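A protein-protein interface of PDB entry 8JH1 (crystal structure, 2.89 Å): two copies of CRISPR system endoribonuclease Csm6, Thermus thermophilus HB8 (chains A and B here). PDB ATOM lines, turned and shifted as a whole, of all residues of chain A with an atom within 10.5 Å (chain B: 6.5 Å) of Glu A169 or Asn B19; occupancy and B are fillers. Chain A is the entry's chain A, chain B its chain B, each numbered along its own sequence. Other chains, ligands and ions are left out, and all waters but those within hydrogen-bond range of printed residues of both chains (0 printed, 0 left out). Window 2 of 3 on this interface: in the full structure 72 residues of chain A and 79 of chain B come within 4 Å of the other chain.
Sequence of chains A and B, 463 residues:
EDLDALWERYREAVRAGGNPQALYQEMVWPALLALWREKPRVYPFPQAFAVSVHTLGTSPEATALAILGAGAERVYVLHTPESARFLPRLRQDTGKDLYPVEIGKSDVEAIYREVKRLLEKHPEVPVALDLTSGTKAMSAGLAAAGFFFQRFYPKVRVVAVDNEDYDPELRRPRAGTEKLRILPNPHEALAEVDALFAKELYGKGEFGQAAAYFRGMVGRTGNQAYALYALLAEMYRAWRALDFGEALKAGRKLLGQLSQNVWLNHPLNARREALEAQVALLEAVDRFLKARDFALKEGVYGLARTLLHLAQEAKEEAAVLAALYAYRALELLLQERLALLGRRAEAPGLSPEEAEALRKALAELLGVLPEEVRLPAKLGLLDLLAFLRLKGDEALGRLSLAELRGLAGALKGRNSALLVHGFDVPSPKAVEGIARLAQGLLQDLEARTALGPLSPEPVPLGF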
ATOM      1  N   TRP A   7       1.788  37.677   0.410  1.00  0.00           N
ATOM      2  CA  TRP A   7       1.752  36.498  -0.445  1.00  0.00           C
ATOM      3  C   TRP A   7       0.535  35.639  -0.133  1.00  0.00           C
ATOM      4  O   TRP A   7      -0.121  35.123  -1.045  1.00  0.00           O
ATOM      5  CB  TRP A   7       3.046  35.688  -0.298  1.00  0.00           C
ATOM      6  CG  TRP A   7       3.009  34.362  -1.006  1.00  0.00           C
ATOM      7  CD1 TRP A   7       2.750  33.160  -0.449  1.00  0.00           C
ATOM      8  CD2 TRP A   7       3.238  34.114  -2.403  1.00  0.00           C
ATOM      9  NE1 TRP A   7       2.788  32.172  -1.399  1.00  0.00           N
ATOM     10  CE2 TRP A   7       3.084  32.731  -2.608  1.00  0.00           C
ATOM     11  CE3 TRP A   7       3.544  34.932  -3.498  1.00  0.00           C
ATOM     12  CZ2 TRP A   7       3.236  32.136  -3.852  1.00  0.00           C
ATOM     13  CZ3 TRP A   7       3.694  34.343  -4.743  1.00  0.00           C
ATOM     14  CH2 TRP A   7       3.542  32.953  -4.909  1.00  0.00           C
ATOM     15  N   TYR A  10      -2.366  37.453  -1.694  1.00  0.00           N
ATOM     16  CA  TYR A  10      -2.365  37.272  -3.137  1.00  0.00           C
ATOM     17  C   TYR A  10      -2.870  35.883  -3.506  1.00  0.00           C
ATOM     18  O   TYR A  10      -3.630  35.721  -4.472  1.00  0.00           O
ATOM     19  CB  TYR A  10      -0.959  37.526  -3.679  1.00  0.00           C
ATOM     20  CG  TYR A  10      -0.674  36.888  -5.011  1.00  0.00           C
ATOM     21  CD1 TYR A  10      -1.285  37.343  -6.172  1.00  0.00           C
ATOM     22  CD2 TYR A  10       0.219  35.841  -5.111  1.00  0.00           C
ATOM     23  CE1 TYR A  10      -1.021  36.761  -7.394  1.00  0.00           C
ATOM     24  CE2 TYR A  10       0.490  35.246  -6.328  1.00  0.00           C
ATOM     25  CZ  TYR A  10      -0.133  35.703  -7.471  1.00  0.00           C
ATOM     26  OH  TYR A  10       0.162  35.097  -8.688  1.00  0.00           O
ATOM     27  N   ARG A  11      -2.477  34.867  -2.736  1.00  0.00           N
ATOM     28  CA  ARG A  11      -3.033  33.532  -2.936  1.00  0.00           C
ATOM     29  C   ARG A  11      -4.542  33.532  -2.736  1.00  0.00           C
ATOM     30  O   ARG A  11      -5.294  33.013  -3.569  1.00  0.00           O
ATOM     31  CB  ARG A  11      -2.368  32.545  -1.982  1.00  0.00           C
ATOM     32  CG  ARG A  11      -1.042  32.049  -2.466  1.00  0.00           C
ATOM     33  CD  ARG A  11      -0.314  31.310  -1.368  1.00  0.00           C
ATOM     34  NE  ARG A  11      -1.117  30.271  -0.726  1.00  0.00           N
ATOM     35  CZ  ARG A  11      -1.508  29.142  -1.308  1.00  0.00           C
ATOM     36  NH1 ARG A  11      -1.276  28.901  -2.596  1.00  0.00           N
ATOM     37  NH2 ARG A  11      -2.138  28.225  -0.576  1.00  0.00           N
ATOM     38  N   GLU A  12      -4.996  34.121  -1.631  1.00  0.00           N
ATOM     39  CA  GLU A  12      -6.418  34.262  -1.352  1.00  0.00           C
ATOM     40  C   GLU A  12      -7.149  34.882  -2.532  1.00  0.00           C
ATOM     41  O   GLU A  12      -8.260  34.464  -2.880  1.00  0.00           O
ATOM     42  CB  GLU A  12      -6.593  35.135  -0.112  1.00  0.00           C
ATOM     43  CG  GLU A  12      -8.010  35.322   0.377  1.00  0.00           C
ATOM     44  CD  GLU A  12      -8.091  35.340   1.891  1.00  0.00           C
ATOM     45  OE1 GLU A  12      -7.097  34.964   2.560  1.00  0.00           O
ATOM     46  OE2 GLU A  12      -9.135  35.783   2.415  1.00  0.00           O
ATOM     47  N   ALA A  13      -6.535  35.895  -3.146  1.00  0.00           N
ATOM     48  CA  ALA A  13      -7.167  36.626  -4.238  1.00  0.00           C
ATOM     49  C   ALA A  13      -7.242  35.782  -5.505  1.00  0.00           C
ATOM     50  O   ALA A  13      -8.279  35.764  -6.179  1.00  0.00           O
ATOM     51  CB  ALA A  13      -6.407  37.925  -4.489  1.00  0.00           C
ATOM     52  N   VAL A  14      -6.155  35.076  -5.840  1.00  0.00           N
ATOM     53  CA  VAL A  14      -6.161  34.227  -7.036  1.00  0.00           C
ATOM     54  C   VAL A  14      -7.146  33.073  -6.877  1.00  0.00           C
ATOM     55  O   VAL A  14      -7.896  32.751  -7.807  1.00  0.00           O
ATOM     56  CB  VAL A  14      -4.750  33.704  -7.364  1.00  0.00           C
ATOM     57  CG1 VAL A  14      -4.744  33.130  -8.754  1.00  0.00           C
ATOM     58  CG2 VAL A  14      -3.749  34.809  -7.309  1.00  0.00           C
ATOM     59  N   ARG A  15      -7.149  32.416  -5.707  1.00  0.00           N
ATOM     60  CA  ARG A  15      -8.052  31.283  -5.512  1.00  0.00           C
ATOM     61  C   ARG A  15      -9.503  31.711  -5.685  1.00  0.00           C
ATOM     62  O   ARG A  15     -10.340  30.924  -6.157  1.00  0.00           O
ATOM     63  CB  ARG A  15      -7.814  30.641  -4.139  1.00  0.00           C
ATOM     64  CG  ARG A  15      -8.636  31.201  -2.987  1.00  0.00           C
ATOM     65  CD  ARG A  15      -9.072  30.086  -2.034  1.00  0.00           C
ATOM     66  NE  ARG A  15      -9.983  30.578  -1.004  1.00  0.00           N
ATOM     67  CZ  ARG A  15     -10.498  29.836  -0.030  1.00  0.00           C
ATOM     68  NH1 ARG A  15     -10.239  28.539   0.064  1.00  0.00           N
ATOM     69  NH2 ARG A  15     -11.283  30.409   0.878  1.00  0.00           N
ATOM     70  N   ALA A  16      -9.802  32.965  -5.358  1.00  0.00           N
ATOM     71  CA  ALA A  16     -11.083  33.585  -5.675  1.00  0.00           C
ATOM     72  C   ALA A  16     -10.983  34.373  -6.979  1.00  0.00           C
ATOM     73  O   ALA A  16     -11.090  35.592  -7.000  1.00  0.00           O
ATOM     74  CB  ALA A  16     -11.537  34.479  -4.525  1.00  0.00           C
ATOM     75  N   GLY A  17     -10.720  33.653  -8.072  1.00  0.00           N
ATOM     76  CA  GLY A  17     -10.966  34.143  -9.418  1.00  0.00           C
ATOM     77  C   GLY A  17     -10.042  35.218  -9.966  1.00  0.00           C
ATOM     78  O   GLY A  17     -10.107  35.497 -11.172  1.00  0.00           O
ATOM     79  N   GLY A  18      -9.187  35.832  -9.147  1.00  0.00           N
ATOM     80  CA  GLY A  18      -8.351  36.911  -9.643  1.00  0.00           C
ATOM     81  C   GLY A  18      -7.347  36.439 -10.681  1.00  0.00           C
ATOM     82  O   GLY A  18      -6.942  35.273 -10.709  1.00  0.00           O
ATOM     83  N   PRO A  20      -3.863  35.827 -11.847  1.00  0.00           N
ATOM     84  CA  PRO A  20      -2.602  35.684 -11.101  1.00  0.00           C
ATOM     85  C   PRO A  20      -1.515  36.652 -11.543  1.00  0.00           C
ATOM     86  O   PRO A  20      -0.750  37.126 -10.700  1.00  0.00           O
ATOM     87  CB  PRO A  20      -2.197  34.229 -11.363  1.00  0.00           C
ATOM     88  CG  PRO A  20      -3.355  33.588 -12.062  1.00  0.00           C
ATOM     89  CD  PRO A  20      -4.125  34.671 -12.717  1.00  0.00           C
ATOM     90  N   GLN A  21      -1.434  36.984 -12.829  1.00  0.00           N
ATOM     91  CA  GLN A  21      -0.346  37.836 -13.308  1.00  0.00           C
ATOM     92  C   GLN A  21      -0.531  39.285 -12.887  1.00  0.00           C
ATOM     93  O   GLN A  21       0.393  39.907 -12.340  1.00  0.00           O
ATOM     94  CB  GLN A  21      -0.229  37.757 -14.830  1.00  0.00           C
ATOM     95  CG  GLN A  21       0.641  38.845 -15.378  1.00  0.00           C
ATOM     96  CD  GLN A  21       1.549  38.343 -16.461  1.00  0.00           C
ATOM     97  OE1 GLN A  21       1.083  37.944 -17.532  1.00  0.00           O
ATOM     98  NE2 GLN A  21       2.867  38.341 -16.190  1.00  0.00           N
ATOM     99  N   ASP A 165      10.964  27.897  -2.111  1.00  0.00           N
ATOM    100  CA  ASP A 165       9.578  27.419  -2.082  1.00  0.00           C
ATOM    101  C   ASP A 165       8.902  27.803  -3.396  1.00  0.00           C
ATOM    102  O   ASP A 165       8.625  28.985  -3.613  1.00  0.00           O
ATOM    103  CB  ASP A 165       8.822  28.005  -0.892  1.00  0.00           C
ATOM    104  CG  ASP A 165       7.402  27.440  -0.762  1.00  0.00           C
ATOM    105  OD1 ASP A 165       7.198  26.260  -1.133  1.00  0.00           O
ATOM    106  OD2 ASP A 165       6.493  28.156  -0.275  1.00  0.00           O
ATOM    107  N   TYR A 166       8.593  26.824  -4.246  1.00  0.00           N
ATOM    108  CA  TYR A 166       7.976  27.104  -5.535  1.00  0.00           C
ATOM    109  C   TYR A 166       6.527  26.646  -5.510  1.00  0.00           C
ATOM    110  O   TYR A 166       6.258  25.460  -5.302  1.00  0.00           O
ATOM    111  CB  TYR A 166       8.738  26.408  -6.655  1.00  0.00           C
ATOM    112  CG  TYR A 166       8.214  26.678  -8.057  1.00  0.00           C
ATOM    113  CD1 TYR A 166       8.552  27.845  -8.747  1.00  0.00           C
ATOM    114  CD2 TYR A 166       7.407  25.752  -8.702  1.00  0.00           C
ATOM    115  CE1 TYR A 166       8.075  28.077 -10.048  1.00  0.00           C
ATOM    116  CE2 TYR A 166       6.938  25.974  -9.972  1.00  0.00           C
ATOM    117  CZ  TYR A 166       7.275  27.124 -10.639  1.00  0.00           C
ATOM    118  OH  TYR A 166       6.801  27.300 -11.895  1.00  0.00           O
ATOM    119  N   ASP A 167       5.592  27.586  -5.733  1.00  0.00           N
ATOM    120  CA  ASP A 167       4.174  27.231  -5.764  1.00  0.00           C
ATOM    121  C   ASP A 167       3.871  26.498  -7.072  1.00  0.00           C
ATOM    122  O   ASP A 167       3.738  27.132  -8.124  1.00  0.00           O
ATOM    123  CB  ASP A 167       3.291  28.482  -5.608  1.00  0.00           C
ATOM    124  CG  ASP A 167       1.931  28.179  -4.940  1.00  0.00           C
ATOM    125  OD1 ASP A 167       0.972  27.760  -5.648  1.00  0.00           O
ATOM    126  OD2 ASP A 167       1.818  28.380  -3.704  1.00  0.00           O
ATOM    127  N   PRO A 168       3.739  25.167  -7.047  1.00  0.00           N
ATOM    128  CA  PRO A 168       3.578  24.420  -8.308  1.00  0.00           C
ATOM    129  C   PRO A 168       2.293  24.736  -9.024  1.00  0.00           C
ATOM    130  O   PRO A 168       2.180  24.474 -10.233  1.00  0.00           O
ATOM    131  CB  PRO A 168       3.591  22.967  -7.847  1.00  0.00           C
ATOM    132  CG  PRO A 168       2.977  23.038  -6.482  1.00  0.00           C
ATOM    133  CD  PRO A 168       3.444  24.340  -5.869  1.00  0.00           C
ATOM    134  N   GLU A 169       1.320  25.271  -8.298  1.00  0.00           N
ATOM    135  CA  GLU A 169      -0.014  25.586  -8.785  1.00  0.00           C
ATOM    136  C   GLU A 169      -0.085  26.988  -9.379  1.00  0.00           C
ATOM    137  O   GLU A 169      -0.673  27.183 -10.454  1.00  0.00           O
ATOM    138  CB  GLU A 169      -0.994  25.446  -7.628  1.00  0.00           C
ATOM    139  CG  GLU A 169      -2.410  25.341  -8.045  1.00  0.00           C
ATOM    140  CD  GLU A 169      -3.260  26.253  -7.199  1.00  0.00           C
ATOM    141  OE1 GLU A 169      -3.159  26.173  -5.953  1.00  0.00           O
ATOM    142  OE2 GLU A 169      -3.984  27.088  -7.792  1.00  0.00           O
ATOM    143  N   LEU A 170       0.510  27.965  -8.686  1.00  0.00           N
ATOM    144  CA  LEU A 170       0.829  29.263  -9.263  1.00  0.00           C
ATOM    145  C   LEU A 170       1.959  29.203 -10.279  1.00  0.00           C
ATOM    146  O   LEU A 170       2.227  30.211 -10.945  1.00  0.00           O
ATOM    147  CB  LEU A 170       1.219  30.246  -8.171  1.00  0.00           C
ATOM    148  CG  LEU A 170       0.149  30.490  -7.133  1.00  0.00           C
ATOM    149  CD1 LEU A 170       0.651  31.523  -6.149  1.00  0.00           C
ATOM    150  CD2 LEU A 170      -1.129  30.912  -7.817  1.00  0.00           C
ATOM    151  N   ARG A 171       2.636  28.070 -10.397  1.00  0.00           N
ATOM    152  CA  ARG A 171       3.835  27.939 -11.211  1.00  0.00           C
ATOM    153  C   ARG A 171       4.751  29.153 -11.054  1.00  0.00           C
ATOM    154  O   ARG A 171       5.239  29.729 -12.026  1.00  0.00           O
ATOM    155  CB  ARG A 171       3.464  27.684 -12.666  1.00  0.00           C
ATOM    156  CG  ARG A 171       2.340  26.669 -12.827  1.00  0.00           C
ATOM    157  CD  ARG A 171       1.893  26.567 -14.269  1.00  0.00           C
ATOM    158  NE  ARG A 171       2.975  26.139 -15.135  1.00  0.00           N
ATOM    159  CZ  ARG A 171       3.321  24.873 -15.319  1.00  0.00           C
ATOM    160  NH1 ARG A 171       2.664  23.887 -14.729  1.00  0.00           N
ATOM    161  NH2 ARG A 171       4.348  24.588 -16.118  1.00  0.00           N
ATOM    162  N   ARG A 172       4.994  29.525  -9.804  1.00  0.00           N
ATOM    163  CA  ARG A 172       5.754  30.707  -9.411  1.00  0.00           C
ATOM    164  C   ARG A 172       6.550  30.367  -8.150  1.00  0.00           C
ATOM    165  O   ARG A 172       6.183  29.467  -7.417  1.00  0.00           O
ATOM    166  CB  ARG A 172       4.826  31.882  -9.093  1.00  0.00           C
ATOM    167  CG  ARG A 172       5.465  33.239  -9.207  1.00  0.00           C
ATOM    168  CD  ARG A 172       4.432  34.308  -9.085  1.00  0.00           C
ATOM    169  NE  ARG A 172       3.728  34.571 -10.335  1.00  0.00           N
ATOM    170  CZ  ARG A 172       4.192  35.362 -11.296  1.00  0.00           C
ATOM    171  NH1 ARG A 172       5.410  35.886 -11.233  1.00  0.00           N
ATOM    172  NH2 ARG A 172       3.413  35.644 -12.341  1.00  0.00           N
ATOM    173  N   PRO A 173       7.640  31.099  -7.912  1.00  0.00           N
ATOM    174  CA  PRO A 173       8.231  31.054  -6.561  1.00  0.00           C
ATOM    175  C   PRO A 173       7.340  31.788  -5.578  1.00  0.00           C
ATOM    176  O   PRO A 173       6.782  32.840  -5.898  1.00  0.00           O
ATOM    177  CB  PRO A 173       9.568  31.785  -6.735  1.00  0.00           C
ATOM    178  CG  PRO A 173       9.830  31.799  -8.190  1.00  0.00           C
ATOM    179  CD  PRO A 173       8.496  31.797  -8.869  1.00  0.00           C
ATOM    180  N   ARG A 174       7.208  31.236  -4.369  1.00  0.00           N
ATOM    181  CA  ARG A 174       6.611  32.004  -3.283  1.00  0.00           C
ATOM    182  C   ARG A 174       7.495  33.196  -2.981  1.00  0.00           C
ATOM    183  O   ARG A 174       8.703  33.041  -2.787  1.00  0.00           O
ATOM    184  CB  ARG A 174       6.448  31.177  -2.011  1.00  0.00           C
ATOM    185  CG  ARG A 174       6.354  32.056  -0.743  1.00  0.00           C
ATOM    186  CD  ARG A 174       5.649  31.371   0.446  1.00  0.00           C
ATOM    187  NE  ARG A 174       6.380  30.200   0.923  1.00  0.00           N
ATOM    188  CZ  ARG A 174       7.490  30.249   1.654  1.00  0.00           C
ATOM    189  NH1 ARG A 174       7.994  31.401   2.071  1.00  0.00           N
ATOM    190  NH2 ARG A 174       8.107  29.114   1.977  1.00  0.00           N
ATOM    191  N   TYR B  10     -10.528  25.758 -21.948  1.00  0.00           N
ATOM    192  CA  TYR B  10      -9.809  25.656 -20.673  1.00  0.00           C
ATOM    193  C   TYR B  10      -9.452  27.027 -20.118  1.00  0.00           C
ATOM    194  O   TYR B  10      -9.482  27.246 -18.900  1.00  0.00           O
ATOM    195  CB  TYR B  10      -8.526  24.845 -20.830  1.00  0.00           C
ATOM    196  CG  TYR B  10      -7.574  25.034 -19.668  1.00  0.00           C
ATOM    197  CD1 TYR B  10      -7.898  24.548 -18.401  1.00  0.00           C
ATOM    198  CD2 TYR B  10      -6.365  25.695 -19.826  1.00  0.00           C
ATOM    199  CE1 TYR B  10      -7.045  24.704 -17.328  1.00  0.00           C
ATOM    200  CE2 TYR B  10      -5.506  25.861 -18.747  1.00  0.00           C
ATOM    201  CZ  TYR B  10      -5.863  25.363 -17.503  1.00  0.00           C
ATOM    202  OH  TYR B  10      -5.028  25.514 -16.433  1.00  0.00           O
ATOM    203  N   ALA B  13     -12.461  28.277 -18.672  1.00  0.00           N
ATOM    204  CA  ALA B  13     -12.681  27.579 -17.408  1.00  0.00           C
ATOM    205  C   ALA B  13     -11.831  28.155 -16.272  1.00  0.00           C
ATOM    206  O   ALA B  13     -12.313  28.301 -15.143  1.00  0.00           O
ATOM    207  CB  ALA B  13     -12.398  26.089 -17.594  1.00  0.00           C
ATOM    208  N   VAL B  14     -10.562  28.466 -16.538  1.00  0.00           N
ATOM    209  CA  VAL B  14      -9.731  29.044 -15.480  1.00  0.00           C
ATOM    210  C   VAL B  14     -10.223  30.442 -15.125  1.00  0.00           C
ATOM    211  O   VAL B  14     -10.283  30.807 -13.941  1.00  0.00           O
ATOM    212  CB  VAL B  14      -8.239  29.047 -15.873  1.00  0.00           C
ATOM    213  CG1 VAL B  14      -7.424  29.851 -14.870  1.00  0.00           C
ATOM    214  CG2 VAL B  14      -7.706  27.640 -15.924  1.00  0.00           C
ATOM    215  N   GLY B  17     -12.614  30.850 -12.451  1.00  0.00           N
ATOM    216  CA  GLY B  17     -12.156  30.498 -11.121  1.00  0.00           C
ATOM    217  C   GLY B  17     -11.718  29.066 -10.946  1.00  0.00           C
ATOM    218  O   GLY B  17     -11.391  28.666  -9.821  1.00  0.00           O
ATOM    219  N   GLY B  18     -11.695  28.282 -12.022  1.00  0.00           N
ATOM    220  CA  GLY B  18     -11.212  26.916 -11.928  1.00  0.00           C
ATOM    221  C   GLY B  18      -9.729  26.864 -11.617  1.00  0.00           C
ATOM    222  O   GLY B  18      -8.920  27.528 -12.281  1.00  0.00           O
ATOM    223  N   ASN B  19      -9.366  26.070 -10.600  1.00  0.00           N
ATOM    224  CA  ASN B  19      -7.978  25.886 -10.174  1.00  0.00           C
ATOM    225  C   ASN B  19      -7.170  25.325 -11.343  1.00  0.00           C
ATOM    226  O   ASN B  19      -7.522  24.253 -11.859  1.00  0.00           O
ATOM    227  CB  ASN B  19      -7.927  24.924  -8.996  1.00  0.00           C
ATOM    228  CG  ASN B  19      -6.519  24.439  -8.689  1.00  0.00           C
ATOM    229  OD1 ASN B  19      -6.014  23.482  -9.287  1.00  0.00           O
ATOM    230  ND2 ASN B  19      -5.905  25.057  -7.698  1.00  0.00           N
ATOM    231  N   PRO B  20      -6.075  25.991 -11.784  1.00  0.00           N
ATOM    232  CA  PRO B  20      -5.526  25.687 -13.115  1.00  0.00           C
ATOM    233  C   PRO B  20      -4.678  24.419 -13.195  1.00  0.00           C
ATOM    234  O   PRO B  20      -4.711  23.758 -14.238  1.00  0.00           O
ATOM    235  CB  PRO B  20      -4.709  26.946 -13.455  1.00  0.00           C
ATOM    236  CG  PRO B  20      -5.040  27.956 -12.377  1.00  0.00           C
ATOM    237  CD  PRO B  20      -5.383  27.133 -11.175  1.00  0.00           C
ATOM    238  N   GLN B  21      -3.932  24.055 -12.141  1.00  0.00           N
ATOM    239  CA  GLN B  21      -3.197  22.784 -12.131  1.00  0.00           C
ATOM    240  C   GLN B  21      -4.136  21.600 -12.359  1.00  0.00           C
ATOM    241  O   GLN B  21      -4.048  20.886 -13.371  1.00  0.00           O
ATOM    242  CB  GLN B  21      -2.451  22.618 -10.795  1.00  0.00           C
ATOM    243  CG  GLN B  21      -1.366  21.516 -10.719  1.00  0.00           C
ATOM    244  CD  GLN B  21      -0.552  21.357 -12.004  1.00  0.00           C
ATOM    245  OE1 GLN B  21      -1.041  20.828 -13.009  1.00  0.00           O
ATOM    246  NE2 GLN B  21       0.700  21.829 -11.978  1.00  0.00           N
ATOM    247  N   ALA B  22      -5.064  21.387 -11.418  1.00  0.00           N
ATOM    248  CA  ALA B  22      -5.964  20.241 -11.490  1.00  0.00           C
ATOM    249  C   ALA B  22      -6.923  20.348 -12.666  1.00  0.00           C
ATOM    250  O   ALA B  22      -7.204  19.340 -13.330  1.00  0.00           O
ATOM    251  CB  ALA B  22      -6.732  20.097 -10.178  1.00  0.00           C
ATOM    252  N   LEU B  23      -7.451  21.550 -12.932  1.00  0.00           N
ATOM    253  CA  LEU B  23      -8.315  21.724 -14.093  1.00  0.00           C
ATOM    254  C   LEU B  23      -7.592  21.302 -15.358  1.00  0.00           C
ATOM    255  O   LEU B  23      -8.145  20.569 -16.183  1.00  0.00           O
ATOM    256  CB  LEU B  23      -8.788  23.174 -14.223  1.00  0.00           C
ATOM    257  CG  LEU B  23     -10.088  23.492 -14.976  1.00  0.00           C
ATOM    258  CD1 LEU B  23     -11.185  22.465 -14.689  1.00  0.00           C
ATOM    259  CD2 LEU B  23     -10.559  24.928 -14.718  1.00  0.00           C
ATOM    260  N   TYR B  24      -6.342  21.752 -15.520  1.00  0.00           N
ATOM    261  CA  TYR B  24      -5.558  21.365 -16.686  1.00  0.00           C
ATOM    262  C   TYR B  24      -5.409  19.865 -16.755  1.00  0.00           C
ATOM    263  O   TYR B  24      -5.559  19.267 -17.828  1.00  0.00           O
ATOM    264  CB  TYR B  24      -4.182  22.012 -16.633  1.00  0.00           C
ATOM    265  CG  TYR B  24      -3.317  21.785 -17.860  1.00  0.00           C
ATOM    266  CD1 TYR B  24      -3.414  22.623 -18.962  1.00  0.00           C
ATOM    267  CD2 TYR B  24      -2.361  20.760 -17.894  1.00  0.00           C
ATOM    268  CE1 TYR B  24      -2.610  22.444 -20.071  1.00  0.00           C
ATOM    269  CE2 TYR B  24      -1.543  20.568 -19.014  1.00  0.00           C
ATOM    270  CZ  TYR B  24      -1.674  21.424 -20.101  1.00  0.00           C
ATOM    271  OH  TYR B  24      -0.888  21.270 -21.226  1.00  0.00           O
ATOM    272  N   THR B  58       8.082  20.255 -11.203  1.00  0.00           N
ATOM    273  CA  THR B  58       6.700  20.102 -10.797  1.00  0.00           C
ATOM    274  C   THR B  58       5.727  20.261 -11.960  1.00  0.00           C
ATOM    275  O   THR B  58       4.523  20.380 -11.727  1.00  0.00           O
ATOM    276  CB  THR B  58       6.383  21.079  -9.670  1.00  0.00           C
ATOM    277  OG1 THR B  58       6.170  22.381 -10.218  1.00  0.00           O
ATOM    278  CG2 THR B  58       7.552  21.141  -8.701  1.00  0.00           C
ATOM    279  N   LEU B 170      -1.120  31.950 -17.581  1.00  0.00           N
ATOM    280  CA  LEU B 170      -1.134  30.581 -17.078  1.00  0.00           C
ATOM    281  C   LEU B 170       0.263  29.999 -16.895  1.00  0.00           C
ATOM    282  O   LEU B 170       0.397  28.959 -16.233  1.00  0.00           O
ATOM    283  CB  LEU B 170      -1.905  29.674 -18.032  1.00  0.00           C
ATOM    284  CG  LEU B 170      -3.391  29.949 -18.149  1.00  0.00           C
ATOM    285  CD1 LEU B 170      -3.953  29.025 -19.206  1.00  0.00           C
ATOM    286  CD2 LEU B 170      -4.085  29.782 -16.812  1.00  0.00           C
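Positions printed for both chains: 10, 13, 14, 17, 18, 20, 21 and 170. Of the 8 pairs that touch across the chains among the printed residues, none has its exchanged pair printed and touching as well.
Printed residues of chain B within 4 Å of Tyr A166: Thr B58. Glu A169 touches just these residues of chain B: Asn B19, Pro B20 and Gln B21. No residue of chain A comes within 4 Å of Gly B17. Asn B19 touches just one residue of chain A: Glu A169. Of chain A, only Glu A169 (3.7 Å) comes within 4 Å of Pro B20. No residue of chain A comes within 4 Å of Ala B22. No residue of chain A comes within 4 Å of Leu B23. Printed residues of chain A within 4 Å of Thr B58: Tyr A166 and Pro A168. Of the printed residues of chain A, Leu B170 touches Arg A171 (3.4 Å).
The backbone carbonyl oxygen (O) of Pro A168 is in hydrogen-bond range of the side-chain amide nitrogen (NE2) of Gln B21, at 3.5 Å. The side-chain carboxylate (OE2) of Glu A169 sits at hydrogen-bond distance from the side-chain amide nitrogen (ND2) of Asn B19 (2.8 Å).
Printed residues of chain A that touch a printed residue of chain B: Tyr A166, Pro A168, Glu A169 and Arg A171. Of the 13 printed residues of chain B, 5 touch a printed residue of chain A. Among the printed residues, no Asp or Glu carboxylate lies within 4 Å of a Lys or Arg side-chain nitrogen of the other chain.
Among the printed residues, pairs that only touch across the chains: Tyr A166 with Thr B58 (3.7 Å), Pro A168 with Thr B58 (3.6 Å), Glu A169 with Pro B20 (3.7 Å), Glu A169 with Gln B21 (3.9 Å), Arg A171 with Gln B21 (3.96 Å) and Arg A171 with Leu B170 (3.4 Å).
OH of Tyr A166 sits close to O of Arg A171 (2.9 Å). The side-chain hydroxyl (OH) of Tyr B10 sits at hydrogen-bond distance from the backbone carbonyl oxygen (O) of Pro B20, 2.8 Å away. The side-chain amide oxygen of Asn B19 is in hydrogen-bond range of the backbone NH of Ala B22 (3.1 Å).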
